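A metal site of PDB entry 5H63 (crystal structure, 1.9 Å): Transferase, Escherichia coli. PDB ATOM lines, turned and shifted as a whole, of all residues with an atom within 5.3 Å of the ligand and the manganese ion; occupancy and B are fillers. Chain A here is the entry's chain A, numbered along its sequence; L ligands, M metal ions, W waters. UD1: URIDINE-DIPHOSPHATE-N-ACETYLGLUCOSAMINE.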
ATOM      1  N   GLN A  64     -16.935  23.741 -16.959  1.00  0.00           N
ATOM      2  CA  GLN A  64     -16.420  24.992 -17.437  1.00  0.00           C
ATOM      3  C   GLN A  64     -16.030  25.890 -16.265  1.00  0.00           C
ATOM      4  O   GLN A  64     -16.849  26.036 -15.302  1.00  0.00           O
ATOM      5  CB  GLN A  64     -17.483  25.693 -18.286  1.00  0.00           C
ATOM      6  CG  GLN A  64     -17.038  27.068 -18.843  1.00  0.00           C
ATOM      7  CD  GLN A  64     -18.118  27.718 -19.690  1.00  0.00           C
ATOM      8  OE1 GLN A  64     -19.290  27.607 -19.415  1.00  0.00           O
ATOM      9  NE2 GLN A  64     -17.681  28.391 -20.760  1.00  0.00           N
ATOM     10  N   TRP A  65     -14.864  26.538 -16.347  1.00  0.00           N
ATOM     11  CA  TRP A  65     -14.528  27.612 -15.399  1.00  0.00           C
ATOM     12  C   TRP A  65     -13.800  28.759 -16.124  1.00  0.00           C
ATOM     13  O   TRP A  65     -12.606  28.640 -16.432  1.00  0.00           O
ATOM     14  CB  TRP A  65     -13.754  27.163 -14.126  1.00  0.00           C
ATOM     15  CG  TRP A  65     -13.856  28.215 -13.144  1.00  0.00           C
ATOM     16  CD1 TRP A  65     -12.844  29.064 -12.801  1.00  0.00           C
ATOM     17  CD2 TRP A  65     -15.005  28.672 -12.458  1.00  0.00           C
ATOM     18  NE1 TRP A  65     -13.271  29.980 -11.877  1.00  0.00           N
ATOM     19  CE2 TRP A  65     -14.618  29.780 -11.676  1.00  0.00           C
ATOM     20  CE3 TRP A  65     -16.353  28.263 -12.434  1.00  0.00           C
ATOM     21  CZ2 TRP A  65     -15.521  30.484 -10.863  1.00  0.00           C
ATOM     22  CZ3 TRP A  65     -17.250  28.934 -11.643  1.00  0.00           C
ATOM     23  CH2 TRP A  65     -16.826  30.062 -10.845  1.00  0.00           C
ATOM     24  N   PHE A  66     -14.583  29.794 -16.456  1.00  0.00           N
ATOM     25  CA  PHE A  66     -14.067  31.036 -17.013  1.00  0.00           C
ATOM     26  C   PHE A  66     -13.863  32.029 -15.865  1.00  0.00           C
ATOM     27  O   PHE A  66     -14.789  32.397 -15.136  1.00  0.00           O
ATOM     28  CB  PHE A  66     -15.028  31.569 -18.076  1.00  0.00           C
ATOM     29  CG  PHE A  66     -14.898  30.921 -19.423  1.00  0.00           C
ATOM     30  CD1 PHE A  66     -14.364  29.632 -19.574  1.00  0.00           C
ATOM     31  CD2 PHE A  66     -15.223  31.647 -20.581  1.00  0.00           C
ATOM     32  CE1 PHE A  66     -14.229  29.024 -20.833  1.00  0.00           C
ATOM     33  CE2 PHE A  66     -15.057  31.052 -21.853  1.00  0.00           C
ATOM     34  CZ  PHE A  66     -14.557  29.747 -21.969  1.00  0.00           C
ATOM     35  N   GLU A  67     -12.634  32.476 -15.703  1.00  0.00           N
ATOM     36  CA  GLU A  67     -12.286  33.193 -14.487  1.00  0.00           C
ATOM     37  C   GLU A  67     -11.892  34.608 -14.840  1.00  0.00           C
ATOM     38  O   GLU A  67     -10.836  34.815 -15.436  1.00  0.00           O
ATOM     39  CB  GLU A  67     -11.151  32.448 -13.772  1.00  0.00           C
ATOM     40  CG  GLU A  67     -10.658  33.193 -12.525  1.00  0.00           C
ATOM     41  CD  GLU A  67     -11.767  33.570 -11.563  1.00  0.00           C
ATOM     42  OE1 GLU A  67     -11.938  34.773 -11.283  1.00  0.00           O
ATOM     43  OE2 GLU A  67     -12.487  32.684 -11.047  1.00  0.00           O
ATOM     44  N   ARG A  72      -7.324  36.760  -7.827  1.00  0.00           N
ATOM     45  CA  ARG A  72      -7.905  36.419  -6.544  1.00  0.00           C
ATOM     46  C   ARG A  72      -7.482  35.039  -5.966  1.00  0.00           C
ATOM     47  O   ARG A  72      -7.726  34.721  -4.798  1.00  0.00           O
ATOM     48  CB  ARG A  72      -9.431  36.613  -6.599  1.00  0.00           C
ATOM     49  CG  ARG A  72     -10.249  35.445  -7.142  1.00  0.00           C
ATOM     50  CD  ARG A  72     -11.651  35.913  -7.523  1.00  0.00           C
ATOM     51  NE  ARG A  72     -12.347  34.864  -8.290  1.00  0.00           N
ATOM     52  CZ  ARG A  72     -13.479  34.262  -7.956  1.00  0.00           C
ATOM     53  NH1 ARG A  72     -14.150  34.609  -6.857  1.00  0.00           N
ATOM     54  NH2 ARG A  72     -13.964  33.307  -8.775  1.00  0.00           N
ATOM     55  N   ASN A  86     -19.424  27.653  -2.802  1.00  0.00           N
ATOM     56  CA  ASN A  86     -19.231  27.232  -4.220  1.00  0.00           C
ATOM     57  C   ASN A  86     -18.022  26.270  -4.311  1.00  0.00           C
ATOM     58  O   ASN A  86     -16.945  26.688  -4.726  1.00  0.00           O
ATOM     59  CB  ASN A  86     -19.013  28.451  -5.108  1.00  0.00           C
ATOM     60  CG  ASN A  86     -20.245  29.355  -5.191  1.00  0.00           C
ATOM     61  OD1 ASN A  86     -20.153  30.501  -4.795  1.00  0.00           O
ATOM     62  ND2 ASN A  86     -21.355  28.849  -5.674  1.00  0.00           N
ATOM     63  N   TYR A  88     -16.613  24.258  -6.186  1.00  0.00           N
ATOM     64  CA  TYR A  88     -16.679  23.724  -7.570  1.00  0.00           C
ATOM     65  C   TYR A  88     -15.537  22.822  -8.025  1.00  0.00           C
ATOM     66  O   TYR A  88     -15.767  21.807  -8.670  1.00  0.00           O
ATOM     67  CB  TYR A  88     -17.028  24.832  -8.543  1.00  0.00           C
ATOM     68  CG  TYR A  88     -18.423  25.471  -8.395  1.00  0.00           C
ATOM     69  CD1 TYR A  88     -19.369  25.001  -7.484  1.00  0.00           C
ATOM     70  CD2 TYR A  88     -18.780  26.580  -9.151  1.00  0.00           C
ATOM     71  CE1 TYR A  88     -20.642  25.561  -7.368  1.00  0.00           C
ATOM     72  CE2 TYR A  88     -20.066  27.116  -9.076  1.00  0.00           C
ATOM     73  CZ  TYR A  88     -20.978  26.629  -8.113  1.00  0.00           C
ATOM     74  OH  TYR A  88     -22.234  27.226  -7.994  1.00  0.00           O
ATOM     75  N   HIS A 200     -21.805  36.970 -17.413  1.00  0.00           N
ATOM     76  CA  HIS A 200     -22.176  35.586 -17.703  1.00  0.00           C
ATOM     77  C   HIS A 200     -22.224  35.275 -19.200  1.00  0.00           C
ATOM     78  O   HIS A 200     -22.094  34.127 -19.591  1.00  0.00           O
ATOM     79  CB  HIS A 200     -23.515  35.171 -17.065  1.00  0.00           C
ATOM     80  CG  HIS A 200     -24.699  35.836 -17.670  1.00  0.00           C
ATOM     81  ND1 HIS A 200     -25.431  35.265 -18.673  1.00  0.00           N
ATOM     82  CD2 HIS A 200     -25.213  37.074 -17.491  1.00  0.00           C
ATOM     83  CE1 HIS A 200     -26.376  36.110 -19.051  1.00  0.00           C
ATOM     84  NE2 HIS A 200     -26.272  37.210 -18.346  1.00  0.00           N
ATOM     85  N   PHE A 203     -18.937  33.180 -20.552  1.00  0.00           N
ATOM     86  CA  PHE A 203     -18.978  31.703 -20.454  1.00  0.00           C
ATOM     87  C   PHE A 203     -20.170  31.087 -21.175  1.00  0.00           C
ATOM     88  O   PHE A 203     -20.002  30.046 -21.829  1.00  0.00           O
ATOM     89  CB  PHE A 203     -18.780  31.143 -19.049  1.00  0.00           C
ATOM     90  CG  PHE A 203     -19.508  31.848 -17.955  1.00  0.00           C
ATOM     91  CD1 PHE A 203     -18.882  32.840 -17.231  1.00  0.00           C
ATOM     92  CD2 PHE A 203     -20.732  31.424 -17.568  1.00  0.00           C
ATOM     93  CE1 PHE A 203     -19.520  33.440 -16.140  1.00  0.00           C
ATOM     94  CE2 PHE A 203     -21.385  31.964 -16.482  1.00  0.00           C
ATOM     95  CZ  PHE A 203     -20.801  32.990 -15.763  1.00  0.00           C
ATOM     96  N   ASP A 204     -21.336  31.702 -21.133  1.00  0.00           N
ATOM     97  CA  ASP A 204     -22.514  31.115 -21.822  1.00  0.00           C
ATOM     98  C   ASP A 204     -22.330  30.985 -23.334  1.00  0.00           C
ATOM     99  O   ASP A 204     -22.677  29.953 -23.928  1.00  0.00           O
ATOM    100  CB  ASP A 204     -23.808  31.846 -21.494  1.00  0.00           C
ATOM    101  CG  ASP A 204     -24.262  31.601 -20.088  1.00  0.00           C
ATOM    102  OD1 ASP A 204     -23.618  30.781 -19.367  1.00  0.00           O
ATOM    103  OD2 ASP A 204     -25.224  32.266 -19.705  1.00  0.00           O
ATOM    104  N   ARG A 207     -19.503  28.334 -24.108  1.00  0.00           N
ATOM    105  CA  ARG A 207     -20.012  26.963 -23.831  1.00  0.00           C
ATOM    106  C   ARG A 207     -20.699  26.368 -25.078  1.00  0.00           C
ATOM    107  O   ARG A 207     -20.420  25.236 -25.457  1.00  0.00           O
ATOM    108  CB  ARG A 207     -20.921  27.009 -22.593  1.00  0.00           C
ATOM    109  CG  ARG A 207     -21.517  25.663 -22.209  1.00  0.00           C
ATOM    110  CD  ARG A 207     -22.474  25.851 -21.071  1.00  0.00           C
ATOM    111  NE  ARG A 207     -21.881  26.609 -19.965  1.00  0.00           N
ATOM    112  CZ  ARG A 207     -22.583  27.157 -18.975  1.00  0.00           C
ATOM    113  NH1 ARG A 207     -23.899  27.151 -18.967  1.00  0.00           N
ATOM    114  NH2 ARG A 207     -21.924  27.844 -18.020  1.00  0.00           N
ATOM    115  N   TYR A 237     -22.073  18.344 -21.120  1.00  0.00           N
ATOM    116  CA  TYR A 237     -21.762  19.552 -20.362  1.00  0.00           C
ATOM    117  C   TYR A 237     -22.586  19.610 -19.084  1.00  0.00           C
ATOM    118  O   TYR A 237     -23.852  19.482 -19.154  1.00  0.00           O
ATOM    119  CB  TYR A 237     -22.063  20.823 -21.185  1.00  0.00           C
ATOM    120  CG  TYR A 237     -21.918  21.966 -20.278  1.00  0.00           C
ATOM    121  CD1 TYR A 237     -20.675  22.443 -19.938  1.00  0.00           C
ATOM    122  CD2 TYR A 237     -23.039  22.452 -19.594  1.00  0.00           C
ATOM    123  CE1 TYR A 237     -20.558  23.425 -18.960  1.00  0.00           C
ATOM    124  CE2 TYR A 237     -22.931  23.406 -18.612  1.00  0.00           C
ATOM    125  CZ  TYR A 237     -21.684  23.911 -18.313  1.00  0.00           C
ATOM    126  OH  TYR A 237     -21.570  24.872 -17.303  1.00  0.00           O
ATOM    127  N   LEU A 238     -21.916  19.900 -17.985  1.00  0.00           N
ATOM    128  CA  LEU A 238     -22.557  20.108 -16.650  1.00  0.00           C
ATOM    129  C   LEU A 238     -22.002  21.332 -15.982  1.00  0.00           C
ATOM    130  O   LEU A 238     -20.749  21.495 -15.914  1.00  0.00           O
ATOM    131  CB  LEU A 238     -22.309  18.923 -15.713  1.00  0.00           C
ATOM    132  CG  LEU A 238     -22.734  17.560 -16.138  1.00  0.00           C
ATOM    133  CD1 LEU A 238     -22.166  16.577 -15.135  1.00  0.00           C
ATOM    134  CD2 LEU A 238     -24.205  17.322 -16.276  1.00  0.00           C
ATOM    135  N   ASP A 239     -22.886  22.153 -15.451  1.00  0.00           N
ATOM    136  CA  ASP A 239     -22.532  23.149 -14.433  1.00  0.00           C
ATOM    137  C   ASP A 239     -21.825  22.410 -13.253  1.00  0.00           C
ATOM    138  O   ASP A 239     -22.206  21.312 -12.878  1.00  0.00           O
ATOM    139  CB  ASP A 239     -23.782  23.853 -13.891  1.00  0.00           C
ATOM    140  CG  ASP A 239     -24.322  24.977 -14.808  1.00  0.00           C
ATOM    141  OD1 ASP A 239     -23.716  25.290 -15.878  1.00  0.00           O
ATOM    142  OD2 ASP A 239     -25.343  25.610 -14.428  1.00  0.00           O
ATOM    143  N   ALA A 240     -20.853  23.051 -12.642  1.00  0.00           N
ATOM    144  CA  ALA A 240     -20.036  22.449 -11.602  1.00  0.00           C
ATOM    145  C   ALA A 240     -20.776  22.168 -10.304  1.00  0.00           C
ATOM    146  O   ALA A 240     -20.256  21.465  -9.479  1.00  0.00           O
ATOM    147  CB  ALA A 240     -18.800  23.312 -11.352  1.00  0.00           C
ATOM    148  N   ASP A 241     -22.010  22.667 -10.141  1.00  0.00           N
ATOM    149  CA  ASP A 241     -22.854  22.305  -9.003  1.00  0.00           C
ATOM    150  C   ASP A 241     -23.880  21.169  -9.300  1.00  0.00           C
ATOM    151  O   ASP A 241     -24.782  20.955  -8.491  1.00  0.00           O
ATOM    152  CB  ASP A 241     -23.587  23.563  -8.563  1.00  0.00           C
ATOM    153  CG  ASP A 241     -24.688  24.005  -9.578  1.00  0.00           C
ATOM    154  OD1 ASP A 241     -24.696  23.556 -10.766  1.00  0.00           O
ATOM    155  OD2 ASP A 241     -25.476  24.869  -9.179  1.00  0.00           O
ATOM    156  N   MET A 242     -23.796  20.541 -10.469  1.00  0.00           N
ATOM    157  CA  MET A 242     -24.581  19.384 -10.821  1.00  0.00           C
ATOM    158  C   MET A 242     -23.810  18.170 -10.222  1.00  0.00           C
ATOM    159  O   MET A 242     -22.843  17.661 -10.802  1.00  0.00           O
ATOM    160  CB  MET A 242     -24.707  19.267 -12.375  1.00  0.00           C
ATOM    161  CG  MET A 242     -25.361  20.444 -13.072  1.00  0.00           C
ATOM    162  SD  MET A 242     -27.132  20.418 -12.837  1.00  0.00           S
ATOM    163  CE  MET A 242     -27.705  21.930 -13.652  1.00  0.00           C
ATOM    164  N   HIS A 260     -31.002  20.584 -19.591  1.00  0.00           N
ATOM    165  CA  HIS A 260     -31.605  20.759 -18.289  1.00  0.00           C
ATOM    166  C   HIS A 260     -33.018  21.399 -18.384  1.00  0.00           C
ATOM    167  O   HIS A 260     -33.245  22.345 -19.191  1.00  0.00           O
ATOM    168  CB  HIS A 260     -30.677  21.625 -17.408  1.00  0.00           C
ATOM    169  CG  HIS A 260     -31.134  21.834 -16.010  1.00  0.00           C
ATOM    170  ND1 HIS A 260     -31.621  20.831 -15.204  1.00  0.00           N
ATOM    171  CD2 HIS A 260     -31.061  22.940 -15.231  1.00  0.00           C
ATOM    172  CE1 HIS A 260     -31.872  21.321 -13.997  1.00  0.00           C
ATOM    173  NE2 HIS A 260     -31.536  22.610 -13.993  1.00  0.00           N
ATOM    174  N   GLU A 271     -33.470  25.259 -19.331  1.00  0.00           N
ATOM    175  CA  GLU A 271     -32.406  25.949 -18.607  1.00  0.00           C
ATOM    176  C   GLU A 271     -31.121  25.572 -19.215  1.00  0.00           C
ATOM    177  O   GLU A 271     -30.981  24.546 -19.825  1.00  0.00           O
ATOM    178  CB  GLU A 271     -32.387  25.534 -17.155  1.00  0.00           C
ATOM    179  CG  GLU A 271     -33.666  25.859 -16.412  1.00  0.00           C
ATOM    180  CD  GLU A 271     -33.942  27.329 -16.250  1.00  0.00           C
ATOM    181  OE1 GLU A 271     -35.023  27.596 -15.736  1.00  0.00           O
ATOM    182  OE2 GLU A 271     -33.161  28.211 -16.618  1.00  0.00           O
ATOM    183  N   ASN A 272     -30.171  26.457 -19.034  1.00  0.00           N
ATOM    184  CA  ASN A 272     -28.840  26.149 -19.278  1.00  0.00           C
ATOM    185  C   ASN A 272     -28.398  25.227 -18.123  1.00  0.00           C
ATOM    186  O   ASN A 272     -29.072  25.167 -17.069  1.00  0.00           O
ATOM    187  CB  ASN A 272     -28.056  27.467 -19.314  1.00  0.00           C
ATOM    188  CG  ASN A 272     -26.873  27.351 -20.214  1.00  0.00           C
ATOM    189  OD1 ASN A 272     -26.296  26.229 -20.333  1.00  0.00           O
ATOM    190  ND2 ASN A 272     -26.448  28.458 -20.773  1.00  0.00           N
ATOM    191  N   GLY A 273     -27.270  24.606 -18.256  1.00  0.00           N
ATOM    192  CA  GLY A 273     -26.623  24.008 -17.082  1.00  0.00           C
ATOM    193  C   GLY A 273     -26.380  22.527 -17.217  1.00  0.00           C
ATOM    194  O   GLY A 273     -25.545  21.984 -16.499  1.00  0.00           O
ATOM    195  N   ASN A 338     -28.208  21.610  -9.953  1.00  0.00           N
ATOM    196  CA  ASN A 338     -28.279  23.060  -9.655  1.00  0.00           C
ATOM    197  C   ASN A 338     -28.228  23.297  -8.135  1.00  0.00           C
ATOM    198  O   ASN A 338     -29.087  23.997  -7.562  1.00  0.00           O
ATOM    199  CB  ASN A 338     -29.541  23.724 -10.278  1.00  0.00           C
ATOM    200  CG  ASN A 338     -29.494  25.236 -10.207  1.00  0.00           C
ATOM    201  OD1 ASN A 338     -28.489  25.820  -9.814  1.00  0.00           O
ATOM    202  ND2 ASN A 338     -30.588  25.888 -10.570  1.00  0.00           N
ATOM    203  N   THR A 339     -27.218  22.725  -7.495  1.00  0.00           N
ATOM    204  CA  THR A 339     -27.122  22.872  -6.031  1.00  0.00           C
ATOM    205  C   THR A 339     -26.788  24.271  -5.554  1.00  0.00           C
ATOM    206  O   THR A 339     -27.011  24.596  -4.383  1.00  0.00           O
ATOM    207  CB  THR A 339     -26.169  21.857  -5.393  1.00  0.00           C
ATOM    208  OG1 THR A 339     -24.833  22.035  -5.876  1.00  0.00           O
ATOM    209  CG2 THR A 339     -26.636  20.463  -5.637  1.00  0.00           C
ATOM    210  N   SER A 340     -26.311  25.122  -6.427  1.00  0.00           N
ATOM    211  CA  SER A 340     -26.091  26.506  -6.065  1.00  0.00           C
ATOM    212  C   SER A 340     -27.406  27.230  -5.659  1.00  0.00           C
ATOM    213  O   SER A 340     -27.375  28.097  -4.877  1.00  0.00           O
ATOM    214  CB  SER A 340     -25.412  27.267  -7.189  1.00  0.00           C
ATOM    215  OG  SER A 340     -26.303  27.702  -8.105  1.00  0.00           O
ATOM    216  N   SER A 341     -28.535  26.864  -6.230  1.00  0.00           N
ATOM    217  CA  SER A 341     -29.792  27.528  -5.921  1.00  0.00           C
ATOM    218  C   SER A 341     -30.260  27.224  -4.520  1.00  0.00           C
ATOM    219  O   SER A 341     -31.196  27.791  -4.056  1.00  0.00           O
ATOM    220  CB  SER A 341     -30.859  27.283  -6.950  1.00  0.00           C
ATOM    221  OG  SER A 341     -31.126  25.960  -7.068  1.00  0.00           O
ATOM    222  N   ALA A 344     -25.458  29.423  -2.962  1.00  0.00           N
ATOM    223  CA  ALA A 344     -25.322  30.713  -3.651  1.00  0.00           C
ATOM    224  C   ALA A 344     -24.718  30.680  -5.039  1.00  0.00           C
ATOM    225  O   ALA A 344     -23.727  30.060  -5.280  1.00  0.00           O
ATOM    226  CB  ALA A 344     -24.561  31.728  -2.816  1.00  0.00           C
ATOM    227  N   SER A 345     -25.284  31.505  -5.895  1.00  0.00           N
ATOM    228  CA  SER A 345     -24.797  31.697  -7.286  1.00  0.00           C
ATOM    229  C   SER A 345     -23.350  32.216  -7.287  1.00  0.00           C
ATOM    230  O   SER A 345     -23.003  33.185  -6.579  1.00  0.00           O
ATOM    231  CB  SER A 345     -25.699  32.719  -8.013  1.00  0.00           C
ATOM    232  OG  SER A 345     -26.151  32.242  -9.269  1.00  0.00           O
ATOM    233  N   SER A 346     -22.502  31.581  -8.107  1.00  0.00           N
ATOM    234  CA  SER A 346     -21.083  31.959  -8.194  1.00  0.00           C
ATOM    235  C   SER A 346     -20.833  33.288  -8.932  1.00  0.00           C
ATOM    236  O   SER A 346     -19.688  33.715  -8.960  1.00  0.00           O
ATOM    237  CB  SER A 346     -20.341  30.875  -8.951  1.00  0.00           C
ATOM    238  OG  SER A 346     -21.005  30.693 -10.158  1.00  0.00           O
ATOM    239  N   TRP A 347     -21.864  33.881  -9.572  1.00  0.00           N
ATOM    240  CA  TRP A 347     -21.738  35.129 -10.400  1.00  0.00           C
ATOM    241  C   TRP A 347     -22.919  36.160 -10.332  1.00  0.00           C
ATOM    242  O   TRP A 347     -22.817  37.220 -10.937  1.00  0.00           O
ATOM    243  CB  TRP A 347     -21.538  34.745 -11.890  1.00  0.00           C
ATOM    244  CG  TRP A 347     -22.786  34.117 -12.406  1.00  0.00           C
ATOM    245  CD1 TRP A 347     -23.172  32.819 -12.262  1.00  0.00           C
ATOM    246  CD2 TRP A 347     -23.884  34.810 -12.995  1.00  0.00           C
ATOM    247  NE1 TRP A 347     -24.416  32.642 -12.764  1.00  0.00           N
ATOM    248  CE2 TRP A 347     -24.892  33.848 -13.221  1.00  0.00           C
ATOM    249  CE3 TRP A 347     -24.119  36.160 -13.372  1.00  0.00           C
ATOM    250  CZ2 TRP A 347     -26.110  34.176 -13.838  1.00  0.00           C
ATOM    251  CZ3 TRP A 347     -25.337  36.476 -13.973  1.00  0.00           C
ATOM    252  CH2 TRP A 347     -26.321  35.477 -14.210  1.00  0.00           C
ATOM    253  N   ARG A 348     -24.020  35.861  -9.645  1.00  0.00           N
ATOM    254  CA  ARG A 348     -25.193  36.789  -9.658  1.00  0.00           C
ATOM    255  C   ARG A 348     -25.053  37.946  -8.646  1.00  0.00           C
ATOM    256  O   ARG A 348     -24.782  37.736  -7.458  1.00  0.00           O
ATOM    257  CB  ARG A 348     -26.526  36.032  -9.470  1.00  0.00           C
ATOM    258  CG  ARG A 348     -26.915  35.183 -10.682  1.00  0.00           C
ATOM    259  CD  ARG A 348     -28.193  34.377 -10.425  1.00  0.00           C
ATOM    260  NE  ARG A 348     -28.383  33.303 -11.410  1.00  0.00           N
ATOM    261  CZ  ARG A 348     -28.875  33.448 -12.647  1.00  0.00           C
ATOM    262  NH1 ARG A 348     -29.209  34.659 -13.114  1.00  0.00           N
ATOM    263  NH2 ARG A 348     -28.980  32.386 -13.447  1.00  0.00           N
HETATM  264  C1' UD1 L   1     -26.986  29.566 -14.247  1.00  0.00           C
HETATM  265  C2' UD1 L   1     -27.051  28.395 -15.275  1.00  0.00           C
HETATM  266  C3' UD1 L   1     -25.685  28.236 -15.935  1.00  0.00           C
HETATM  267  C4' UD1 L   1     -25.421  29.561 -16.626  1.00  0.00           C
HETATM  268  C5' UD1 L   1     -25.476  30.712 -15.598  1.00  0.00           C
HETATM  269  C6' UD1 L   1     -25.188  32.067 -16.254  1.00  0.00           C
HETATM  270  C7' UD1 L   1     -28.775  26.780 -14.404  1.00  0.00           C
HETATM  271  C8' UD1 L   1     -29.806  27.772 -14.677  1.00  0.00           C
HETATM  272  N2' UD1 L   1     -27.540  27.133 -14.681  1.00  0.00           N
HETATM  273  O1' UD1 L   1     -25.983  29.345 -13.224  1.00  0.00           O
HETATM  274  O3' UD1 L   1     -25.649  27.148 -16.862  1.00  0.00           O
HETATM  275  O4' UD1 L   1     -24.099  29.661 -17.103  1.00  0.00           O
HETATM  276  O5' UD1 L   1     -26.755  30.763 -14.991  1.00  0.00           O
HETATM  277  O6' UD1 L   1     -26.219  32.325 -17.157  1.00  0.00           O
HETATM  278  O7' UD1 L   1     -29.071  25.636 -13.884  1.00  0.00           O
HETATM  279  N1  UD1 L   1     -19.264  30.144 -14.283  1.00  0.00           N
HETATM  280  C2  UD1 L   1     -17.998  30.553 -14.748  1.00  0.00           C
HETATM  281  N3  UD1 L   1     -17.342  31.559 -14.183  1.00  0.00           N
HETATM  282  C4  UD1 L   1     -17.896  32.224 -13.149  1.00  0.00           C
HETATM  283  C5  UD1 L   1     -19.149  31.862 -12.662  1.00  0.00           C
HETATM  284  C6  UD1 L   1     -19.839  30.801 -13.244  1.00  0.00           C
HETATM  285  O2  UD1 L   1     -17.447  29.920 -15.700  1.00  0.00           O
HETATM  286  O4  UD1 L   1     -17.277  33.196 -12.670  1.00  0.00           O
HETATM  287  C1B UD1 L   1     -19.913  29.024 -14.985  1.00  0.00           C
HETATM  288  C2B UD1 L   1     -19.435  27.685 -14.472  1.00  0.00           C
HETATM  289  O2' UD1 L   1     -19.351  26.804 -15.570  1.00  0.00           O
HETATM  290  C3B UD1 L   1     -20.510  27.292 -13.472  1.00  0.00           C
HETATM  291  C4B UD1 L   1     -21.720  27.890 -14.147  1.00  0.00           C
HETATM  292  O4B UD1 L   1     -21.283  29.112 -14.785  1.00  0.00           O
HETATM  293  O3B UD1 L   1     -20.707  25.903 -13.399  1.00  0.00           O
HETATM  294  C5B UD1 L   1     -22.899  28.092 -13.248  1.00  0.00           C
HETATM  295  O5B UD1 L   1     -22.567  28.719 -12.010  1.00  0.00           O
HETATM  296  PA  UD1 L   1     -23.727  28.586 -10.913  1.00  0.00           P
HETATM  297  O1A UD1 L   1     -23.005  29.073  -9.713  1.00  0.00           O
HETATM  298  O2A UD1 L   1     -24.340  27.232 -10.924  1.00  0.00           O
HETATM  299  O3A UD1 L   1     -24.829  29.711 -11.259  1.00  0.00           O
HETATM  300  PB  UD1 L   1     -26.363  29.543 -11.645  1.00  0.00           P
HETATM  301  O1B UD1 L   1     -27.080  28.340 -11.272  1.00  0.00           O
HETATM  302  O2B UD1 L   1     -27.040  30.826 -11.631  1.00  0.00           O
HETATM  303 MN    MN M   1     -26.357  26.546 -10.284  1.00  0.00          MN
HETATM  304  O   HOH W   1     -26.361  25.236 -11.909  1.00  0.00           O
HETATM  305  O   HOH W   2     -27.650  30.675 -19.869  1.00  0.00           O
HETATM  306  O   HOH W   3     -22.232  25.401 -11.032  1.00  0.00           O
HETATM  307  O   HOH W   4     -15.356  35.198 -13.492  1.00  0.00           O
HETATM  308  O   HOH W   5     -19.336  23.760 -15.450  1.00  0.00           O
HETATM  309  O   HOH W   6     -29.895  28.678 -10.695  1.00  0.00           O
HETATM  310  O   HOH W   7     -17.385  33.899 -10.086  1.00  0.00           O
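NH1 of Arg 207 sits at hydrogen-bond distance from O3' of the ligand (2.7 Å). An oxygen (O4') of the ligand is in hydrogen-bond range of the side-chain carboxylate (OD1) of Asp 204 (2.6 Å). An oxygen (O3B) of the ligand sits at hydrogen-bond distance from the backbone NH (N) of Ala 240. N2' of the ligand sits at hydrogen-bond distance from OD2 of Asp 239. OH of Tyr 237 lies within hydrogen-bond range of O2' of the ligand (3.4 Å). O2B of the ligand lies within salt-bridge range of NE of Arg 348 (2.8 Å). An oxygen (O3') of the ligand sits close to the backbone NH of Gly 273 (3.3 Å). A nitrogen (N2') of the ligand lies close to the backbone carbonyl oxygen (O) of Asn 272, 3.5 Å away. The side-chain hydroxyl (OG) of Ser 346 lies within hydrogen-bond range of an oxygen (O1A) of the ligand, at 2.6 Å. O of Phe 66 lies within hydrogen-bond range of N3 of the ligand, at 2.9 Å. An oxygen (O2) of the ligand is in hydrogen-bond range of the backbone NH (N) of Phe 66, at 3.0 Å. N of Ser 346 lies within hydrogen-bond range of O1A of the ligand (3.0 Å). The indole nitrogen of Trp 347 is in hydrogen-bond range of an oxygen (O3A) of the ligand. OH of Tyr 88 sits at hydrogen-bond distance from O1A of the ligand (2.6 Å). The backbone carbonyl oxygen (O) of Gln 64 sits at hydrogen-bond distance from an oxygen (O2') of the ligand, 2.6 Å away. O6' of the ligand lies within hydrogen-bond range of ND1 of His 200 (3.4 Å). OG of Ser 345 sits at hydrogen-bond distance from O2B of the ligand (2.9 Å).
OH of Tyr 237 sits close to NH2 of Arg 207 (3.1 Å). The side-chain hydroxyl (OG) of Ser 341 is in hydrogen-bond range of the backbone carbonyl oxygen (O) of Asn 338, at 2.9 Å. OD2 of Asp 204 is in hydrogen-bond range of ND1 of His 200 (3.2 Å). The side-chain amide nitrogen of Gln 64 lies within hydrogen-bond range of the backbone carbonyl oxygen of Phe 203 (3.0 Å). The backbone carbonyl oxygen (O) of Gly 273 is in hydrogen-bond range of the backbone NH (N) of Asp 239 (2.9 Å). The side-chain carboxylate (OD1) of Asp 239 is in salt-bridge range of the guanidinium group (NH1) of Arg 207. The side-chain hydroxyl (OH) of Tyr 88 is in hydrogen-bond range of the side-chain amide nitrogen (ND2) of Asn 86 (3.0 Å). SD of Met 242 sits at hydrogen-bond distance from N of Asn 338 (3.3 Å).
Residues that only touch the ligand: Trp 65, Phe 203, Met 242, His 260 and Glu 271. Of the 30 residues printed, 23 come within 4 Å of the ligand. The nearest printed residue that does not touch the ligand is Asn 86 (4.4 Å).
Three residues have an atom within 4 Å of the manganese ion: Asp 241, Asn 338 and Ser 340. Along chain A the residues within 4 Å of the manganese ion span positions 241 to 340.
The manganese ion is bound by water W1, an oxygen (O1B) of the ligand, the side-chain carboxylate (OD2) of Asp 241, an oxygen (O2A) of the ligand, the side-chain amide oxygen (OD1) of Asn 338 and the side-chain hydroxyl (OG) of Ser 340.
Water W7 bridges the backbone carbonyl oxygen (O) of Ser 346 (2.6 Å) and an oxygen (O4) of the ligand (2.7 Å). Water W3 lies within hydrogen-bond range of O3B of the ligand (2.9 Å), N of Asp 241 (2.9 Å) and N of Ala 240 (3.2 Å). Water W4 lies within hydrogen-bond range of an oxygen (O4) of the ligand and the backbone carbonyl oxygen (O) of Phe 66. Water W5 lies within hydrogen-bond range of the backbone carbonyl oxygen of Leu 238 (2.7 Å), the backbone NH of Gln 64 (2.8 Å), an oxygen (O2') of the ligand (3.0 Å), the side-chain hydroxyl of Tyr 237 (3.1 Å) and the backbone NH of Ala 240 (3.3 Å). Water W2 lies within hydrogen-bond range of the side-chain amide nitrogen of Asn 272, the side-chain carboxylate of Asp 204 and an oxygen (O6') of the ligand.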
